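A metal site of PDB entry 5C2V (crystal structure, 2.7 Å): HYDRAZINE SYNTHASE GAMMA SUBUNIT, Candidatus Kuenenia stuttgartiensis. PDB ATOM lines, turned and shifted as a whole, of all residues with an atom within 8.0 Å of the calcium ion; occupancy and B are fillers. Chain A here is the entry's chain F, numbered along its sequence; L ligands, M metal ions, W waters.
A ring nitrogen (ND1) of His 105 sits at hydrogen-bond distance from an oxygen (O3) of the ligand (2.7 Å). N of Arg 104 sits at hydrogen-bond distance from O1 of the ligand (2.6 Å). An oxygen (O4) of the ligand is in salt-bridge range of the guanidinium group (NE) of Arg 104, at 2.7 Å. An oxygen (O3) of the ligand sits close to the backbone NH (N) of His 105 (3.4 Å).
The backbone carbonyl oxygen of His 105 lies within hydrogen-bond range of the backbone NH of Asp 257 (2.7 Å).
Of the 20 residues printed, 3 come within 4 Å of the calcium ion. Along chain A the residues within 4 Å of the calcium ion span positions 100 to 257.
The calcium ion is bound by the side-chain carboxylate of Asp 257 (2.4 Å), water W3 (2.4 Å), the backbone carbonyl oxygen of Pro 102 (2.4 Å), water W2 (2.4 Å) and the backbone carbonyl oxygen of Leu 100 (2.9 Å). Slightly farther from the calcium ion lies water W1 (3.0 Å).
Water W1 lies within hydrogen-bond range of the backbone NH (N) of Arg 104 (3.0 Å), the side-chain amino group (NZ) of Lys 92 (3.3 Å) and an oxygen (O2) of the ligand (3.4 Å).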
ATOM      1  N   LYS A  92      24.832   4.229   4.704  1.00  0.00           N
ATOM      2  CA  LYS A  92      24.539   2.876   5.168  1.00  0.00           C
ATOM      3  C   LYS A  92      25.561   2.338   6.155  1.00  0.00           C
ATOM      4  O   LYS A  92      26.739   2.698   6.118  1.00  0.00           O
ATOM      5  CB  LYS A  92      24.426   1.922   3.977  1.00  0.00           C
ATOM      6  CG  LYS A  92      23.009   1.684   3.491  1.00  0.00           C
ATOM      7  CD  LYS A  92      22.224   0.848   4.487  1.00  0.00           C
ATOM      8  CE  LYS A  92      20.860   0.454   3.930  1.00  0.00           C
ATOM      9  NZ  LYS A  92      20.062  -0.313   4.919  1.00  0.00           N
ATOM     10  N   GLY A  96      28.301  -6.361   8.569  1.00  0.00           N
ATOM     11  CA  GLY A  96      27.356  -7.451   8.383  1.00  0.00           C
ATOM     12  C   GLY A  96      26.372  -7.193   7.262  1.00  0.00           C
ATOM     13  O   GLY A  96      25.153  -7.263   7.463  1.00  0.00           O
ATOM     14  N   GLY A  97      26.892  -6.902   6.077  1.00  0.00           N
ATOM     15  CA  GLY A  97      26.055  -6.650   4.916  1.00  0.00           C
ATOM     16  C   GLY A  97      25.804  -7.890   4.083  1.00  0.00           C
ATOM     17  O   GLY A  97      24.846  -7.940   3.316  1.00  0.00           O
ATOM     18  N   TYR A  99      24.795 -10.691   4.994  1.00  0.00           N
ATOM     19  CA  TYR A  99      23.735 -11.536   5.535  1.00  0.00           C
ATOM     20  C   TYR A  99      22.342 -11.146   5.071  1.00  0.00           C
ATOM     21  O   TYR A  99      21.389 -11.903   5.275  1.00  0.00           O
ATOM     22  CB  TYR A  99      23.790 -11.529   7.063  1.00  0.00           C
ATOM     23  CG  TYR A  99      25.127 -11.947   7.637  1.00  0.00           C
ATOM     24  CD1 TYR A  99      25.515 -13.276   7.640  1.00  0.00           C
ATOM     25  CD2 TYR A  99      25.992 -11.003   8.192  1.00  0.00           C
ATOM     26  CE1 TYR A  99      26.730 -13.657   8.167  1.00  0.00           C
ATOM     27  CE2 TYR A  99      27.207 -11.383   8.718  1.00  0.00           C
ATOM     28  CZ  TYR A  99      27.576 -12.710   8.706  1.00  0.00           C
ATOM     29  OH  TYR A  99      28.786 -13.099   9.231  1.00  0.00           O
ATOM     30  N   LEU A 100      22.202  -9.973   4.469  1.00  0.00           N
ATOM     31  CA  LEU A 100      20.871  -9.473   4.133  1.00  0.00           C
ATOM     32  C   LEU A 100      20.751  -8.790   2.765  1.00  0.00           C
ATOM     33  O   LEU A 100      20.759  -7.570   2.663  1.00  0.00           O
ATOM     34  CB  LEU A 100      20.409  -8.479   5.206  1.00  0.00           C
ATOM     35  CG  LEU A 100      19.998  -9.090   6.541  1.00  0.00           C
ATOM     36  CD1 LEU A 100      19.940  -8.035   7.625  1.00  0.00           C
ATOM     37  CD2 LEU A 100      18.656  -9.800   6.411  1.00  0.00           C
ATOM     38  N   PRO A 101      20.647  -9.600   1.697  1.00  0.00           N
ATOM     39  CA  PRO A 101      20.261  -9.077   0.384  1.00  0.00           C
ATOM     40  C   PRO A 101      18.755  -8.796   0.350  1.00  0.00           C
ATOM     41  O   PRO A 101      18.023  -9.438   1.093  1.00  0.00           O
ATOM     42  CB  PRO A 101      20.632 -10.207  -0.585  1.00  0.00           C
ATOM     43  CG  PRO A 101      21.514 -11.130   0.201  1.00  0.00           C
ATOM     44  CD  PRO A 101      21.053 -11.013   1.615  1.00  0.00           C
ATOM     45  N   PRO A 102      18.299  -7.851  -0.501  1.00  0.00           N
ATOM     46  CA  PRO A 102      19.061  -6.989  -1.411  1.00  0.00           C
ATOM     47  C   PRO A 102      19.717  -5.814  -0.687  1.00  0.00           C
ATOM     48  O   PRO A 102      19.763  -5.794   0.545  1.00  0.00           O
ATOM     49  CB  PRO A 102      17.984  -6.488  -2.382  1.00  0.00           C
ATOM     50  CG  PRO A 102      16.755  -6.449  -1.564  1.00  0.00           C
ATOM     51  CD  PRO A 102      16.858  -7.624  -0.617  1.00  0.00           C
ATOM     52  N   PHE A 103      20.227  -4.846  -1.445  1.00  0.00           N
ATOM     53  CA  PHE A 103      21.087  -3.829  -0.874  1.00  0.00           C
ATOM     54  C   PHE A 103      20.612  -2.382  -1.054  1.00  0.00           C
ATOM     55  O   PHE A 103      19.688  -2.094  -1.826  1.00  0.00           O
ATOM     56  CB  PHE A 103      22.512  -3.973  -1.433  1.00  0.00           C
ATOM     57  CG  PHE A 103      23.126  -5.320  -1.154  1.00  0.00           C
ATOM     58  CD1 PHE A 103      23.519  -5.664   0.132  1.00  0.00           C
ATOM     59  CD2 PHE A 103      23.323  -6.235  -2.173  1.00  0.00           C
ATOM     60  CE1 PHE A 103      24.083  -6.906   0.402  1.00  0.00           C
ATOM     61  CE2 PHE A 103      23.889  -7.478  -1.913  1.00  0.00           C
ATOM     62  CZ  PHE A 103      24.272  -7.802  -0.630  1.00  0.00           C
ATOM     63  N   ARG A 104      21.265  -1.509  -0.308  1.00  0.00           N
ATOM     64  CA  ARG A 104      20.879  -0.132   0.021  1.00  0.00           C
ATOM     65  C   ARG A 104      19.511  -0.018   0.691  1.00  0.00           C
ATOM     66  O   ARG A 104      19.050  -0.965   1.338  1.00  0.00           O
ATOM     67  CB  ARG A 104      20.911   0.726  -1.247  1.00  0.00           C
ATOM     68  CG  ARG A 104      22.289   0.840  -1.883  1.00  0.00           C
ATOM     69  CD  ARG A 104      22.235   1.221  -3.364  1.00  0.00           C
ATOM     70  NE  ARG A 104      21.604   2.512  -3.593  1.00  0.00           N
ATOM     71  CZ  ARG A 104      22.088   3.446  -4.420  1.00  0.00           C
ATOM     72  NH1 ARG A 104      23.221   3.217  -5.071  1.00  0.00           N
ATOM     73  NH2 ARG A 104      21.445   4.590  -4.574  1.00  0.00           N
ATOM     74  N   HIS A 105      18.860   1.132   0.535  1.00  0.00           N
ATOM     75  CA  HIS A 105      17.617   1.398   1.257  1.00  0.00           C
ATOM     76  C   HIS A 105      16.328   1.016   0.533  1.00  0.00           C
ATOM     77  O   HIS A 105      15.421   0.436   1.128  1.00  0.00           O
ATOM     78  CB  HIS A 105      17.570   2.867   1.670  1.00  0.00           C
ATOM     79  CG  HIS A 105      18.458   3.181   2.832  1.00  0.00           C
ATOM     80  ND1 HIS A 105      19.733   3.686   2.691  1.00  0.00           N
ATOM     81  CD2 HIS A 105      18.264   3.029   4.168  1.00  0.00           C
ATOM     82  CE1 HIS A 105      20.277   3.845   3.885  1.00  0.00           C
ATOM     83  NE2 HIS A 105      19.413   3.456   4.797  1.00  0.00           N
ATOM     84  N   GLU A 106      16.261   1.341  -0.751  1.00  0.00           N
ATOM     85  CA  GLU A 106      15.013   1.188  -1.504  1.00  0.00           C
ATOM     86  C   GLU A 106      14.792  -0.270  -1.881  1.00  0.00           C
ATOM     87  O   GLU A 106      15.739  -1.018  -2.094  1.00  0.00           O
ATOM     88  CB  GLU A 106      15.024   2.080  -2.749  1.00  0.00           C
ATOM     89  CG  GLU A 106      15.360   3.532  -2.432  1.00  0.00           C
ATOM     90  CD  GLU A 106      14.805   4.506  -3.459  1.00  0.00           C
ATOM     91  OE1 GLU A 106      14.865   5.726  -3.213  1.00  0.00           O
ATOM     92  OE2 GLU A 106      14.318   4.038  -4.519  1.00  0.00           O
ATOM     93  N   ALA A 118      16.733  -2.122  -4.279  1.00  0.00           N
ATOM     94  CA  ALA A 118      16.725  -3.587  -4.312  1.00  0.00           C
ATOM     95  C   ALA A 118      17.941  -4.133  -5.050  1.00  0.00           C
ATOM     96  O   ALA A 118      17.826  -5.030  -5.879  1.00  0.00           O
ATOM     97  CB  ALA A 118      15.441  -4.091  -4.966  1.00  0.00           C
ATOM     98  N   THR A 119      19.098  -3.570  -4.738  1.00  0.00           N
ATOM     99  CA  THR A 119      20.337  -3.921  -5.435  1.00  0.00           C
ATOM    100  C   THR A 119      20.655  -5.398  -5.258  1.00  0.00           C
ATOM    101  O   THR A 119      20.749  -5.885  -4.136  1.00  0.00           O
ATOM    102  CB  THR A 119      21.510  -3.070  -4.943  1.00  0.00           C
ATOM    103  OG1 THR A 119      21.085  -1.721  -4.750  1.00  0.00           O
ATOM    104  CG2 THR A 119      22.640  -3.089  -5.958  1.00  0.00           C
ATOM    105  N   SER A 202      15.895  -8.917  10.802  1.00  0.00           N
ATOM    106  CA  SER A 202      15.404  -8.259   9.598  1.00  0.00           C
ATOM    107  C   SER A 202      14.573  -9.178   8.719  1.00  0.00           C
ATOM    108  O   SER A 202      14.864 -10.365   8.584  1.00  0.00           O
ATOM    109  CB  SER A 202      16.583  -7.692   8.791  1.00  0.00           C
ATOM    110  OG  SER A 202      16.129  -7.115   7.571  1.00  0.00           O
ATOM    111  N   ALA A 204      14.218  -8.680   5.529  1.00  0.00           N
ATOM    112  CA  ALA A 204      14.871  -8.671   4.218  1.00  0.00           C
ATOM    113  C   ALA A 204      13.855  -8.536   3.093  1.00  0.00           C
ATOM    114  O   ALA A 204      14.050  -9.055   1.994  1.00  0.00           O
ATOM    115  CB  ALA A 204      15.724  -9.926   4.030  1.00  0.00           C
ATOM    116  N   GLN A 205      12.767  -7.828   3.381  1.00  0.00           N
ATOM    117  CA  GLN A 205      11.704  -7.601   2.405  1.00  0.00           C
ATOM    118  C   GLN A 205      11.375  -6.117   2.318  1.00  0.00           C
ATOM    119  O   GLN A 205      12.046  -5.283   2.926  1.00  0.00           O
ATOM    120  CB  GLN A 205      10.452  -8.404   2.774  1.00  0.00           C
ATOM    121  CG  GLN A 205      10.661  -9.909   2.796  1.00  0.00           C
ATOM    122  CD  GLN A 205       9.414 -10.664   3.216  1.00  0.00           C
ATOM    123  OE1 GLN A 205       8.308 -10.127   3.194  1.00  0.00           O
ATOM    124  NE2 GLN A 205       9.596 -11.919   3.625  1.00  0.00           N
ATOM    125  N   ASP A 257      13.557  -1.330   1.840  1.00  0.00           N
ATOM    126  CA  ASP A 257      14.075  -2.609   2.327  1.00  0.00           C
ATOM    127  C   ASP A 257      14.320  -2.554   3.835  1.00  0.00           C
ATOM    128  O   ASP A 257      14.841  -1.562   4.350  1.00  0.00           O
ATOM    129  CB  ASP A 257      15.354  -2.992   1.590  1.00  0.00           C
ATOM    130  CG  ASP A 257      15.846  -4.382   1.960  1.00  0.00           C
ATOM    131  OD1 ASP A 257      15.000  -5.302   2.066  1.00  0.00           O
ATOM    132  OD2 ASP A 257      17.061  -4.567   2.124  1.00  0.00           O
ATOM    133  N   THR A 258      13.958  -3.631   4.526  1.00  0.00           N
ATOM    134  CA  THR A 258      14.099  -3.680   5.977  1.00  0.00           C
ATOM    135  C   THR A 258      15.555  -3.889   6.399  1.00  0.00           C
ATOM    136  O   THR A 258      16.159  -4.919   6.098  1.00  0.00           O
ATOM    137  CB  THR A 258      13.248  -4.813   6.581  1.00  0.00           C
ATOM    138  OG1 THR A 258      11.866  -4.594   6.263  1.00  0.00           O
ATOM    139  CG2 THR A 258      13.410  -4.860   8.089  1.00  0.00           C
ATOM    140  N   PRO A 259      16.126  -2.898   7.106  1.00  0.00           N
ATOM    141  CA  PRO A 259      17.504  -2.925   7.613  1.00  0.00           C
ATOM    142  C   PRO A 259      17.635  -3.768   8.876  1.00  0.00           C
ATOM    143  O   PRO A 259      16.649  -3.999   9.568  1.00  0.00           O
ATOM    144  CB  PRO A 259      17.806  -1.447   7.898  1.00  0.00           C
ATOM    145  CG  PRO A 259      16.537  -0.679   7.589  1.00  0.00           C
ATOM    146  CD  PRO A 259      15.431  -1.671   7.529  1.00  0.00           C
ATOM    147  N   THR A 260      18.850  -4.222   9.166  1.00  0.00           N
ATOM    148  CA  THR A 260      19.116  -4.987  10.371  1.00  0.00           C
ATOM    149  C   THR A 260      19.052  -4.119  11.618  1.00  0.00           C
ATOM    150  O   THR A 260      19.336  -2.916  11.565  1.00  0.00           O
ATOM    151  CB  THR A 260      20.500  -5.668  10.313  1.00  0.00           C
ATOM    152  OG1 THR A 260      20.721  -6.405  11.525  1.00  0.00           O
ATOM    153  CG2 THR A 260      21.596  -4.636  10.139  1.00  0.00           C
HETATM  154 FE1  LIG L   1      28.264   3.846   0.081  1.00  0.00          FE
HETATM  155  C1  LIG L   1      25.128   2.519   0.528  1.00  0.00           C
HETATM  156  C2  LIG L   1      29.570   0.690  -0.091  1.00  0.00           C
HETATM  157  C3  LIG L   1      31.362   5.152  -0.721  1.00  0.00           C
HETATM  158  C4  LIG L   1      27.169   6.965   0.888  1.00  0.00           C
HETATM  159  N1  LIG L   1      27.479   1.944   0.153  1.00  0.00           N
HETATM  160  C5  LIG L   1      26.177   1.615   0.445  1.00  0.00           C
HETATM  161  C6  LIG L   1      26.109   0.178   0.654  1.00  0.00           C
HETATM  162  C7  LIG L   1      27.335  -0.312   0.480  1.00  0.00           C
HETATM  163  C8  LIG L   1      28.220   0.782   0.159  1.00  0.00           C
HETATM  164  C9  LIG L   1      27.787  -1.793   0.582  1.00  0.00           C
HETATM  165  C10 LIG L   1      24.820  -0.621   0.991  1.00  0.00           C
HETATM  166  C11 LIG L   1      24.899  -1.236   2.396  1.00  0.00           C
HETATM  167  C12 LIG L   1      23.661  -2.037   2.685  1.00  0.00           C
HETATM  168  O1  LIG L   1      22.715  -2.013   1.846  1.00  0.00           O
HETATM  169  O2  LIG L   1      23.606  -2.695   3.750  1.00  0.00           O
HETATM  170  N2  LIG L   1      30.166   3.071  -0.229  1.00  0.00           N
HETATM  171  C13 LIG L   1      30.396   1.733  -0.458  1.00  0.00           C
HETATM  172  C14 LIG L   1      31.663   1.604  -1.158  1.00  0.00           C
HETATM  173  C15 LIG L   1      32.167   2.837  -1.325  1.00  0.00           C
HETATM  174  C16 LIG L   1      31.228   3.780  -0.753  1.00  0.00           C
HETATM  175  C17 LIG L   1      32.305   0.271  -1.601  1.00  0.00           C
HETATM  176  C18 LIG L   1      33.488   3.224  -2.020  1.00  0.00           C
HETATM  177  C19 LIG L   1      33.407   2.981  -3.545  1.00  0.00           C
HETATM  178  N3  LIG L   1      29.120   5.712   0.103  1.00  0.00           N
HETATM  179  C20 LIG L   1      30.399   6.047  -0.300  1.00  0.00           C
HETATM  180  C21 LIG L   1      30.492   7.482  -0.356  1.00  0.00           C
HETATM  181  C22 LIG L   1      29.389   7.978   0.230  1.00  0.00           C
HETATM  182  C23 LIG L   1      28.463   6.879   0.435  1.00  0.00           C
HETATM  183  C24 LIG L   1      31.820   8.250  -0.565  1.00  0.00           C
HETATM  184  C25 LIG L   1      29.082   9.470   0.482  1.00  0.00           C
HETATM  185  C26 LIG L   1      28.850  10.198  -0.868  1.00  0.00           C
HETATM  186  N4  LIG L   1      26.427   4.605   0.701  1.00  0.00           N
HETATM  187  C27 LIG L   1      26.200   5.987   0.784  1.00  0.00           C
HETATM  188  C28 LIG L   1      24.774   6.217   0.745  1.00  0.00           C
HETATM  189  C29 LIG L   1      24.136   4.823   0.630  1.00  0.00           C
HETATM  190  C30 LIG L   1      25.240   3.885   0.616  1.00  0.00           C
HETATM  191  C31 LIG L   1      24.050   7.576   0.798  1.00  0.00           C
HETATM  192  C32 LIG L   1      22.625   4.491   0.548  1.00  0.00           C
HETATM  193  C33 LIG L   1      22.200   4.450  -0.919  1.00  0.00           C
HETATM  194  C34 LIG L   1      20.706   4.310  -0.993  1.00  0.00           C
HETATM  195  O3  LIG L   1      20.048   4.292   0.078  1.00  0.00           O
HETATM  196  O4  LIG L   1      20.161   4.214  -2.127  1.00  0.00           O
HETATM  197 CA    CA M   1      19.263  -5.135   2.779  1.00  0.00          CA
HETATM  198  O   HOH W   1      20.463  -2.418   2.427  1.00  0.00           O
HETATM  199  O   HOH W   2      21.518  -5.615   3.415  1.00  0.00           O
HETATM  200  O   HOH W   3      18.751  -4.591   5.035  1.00  0.00           O
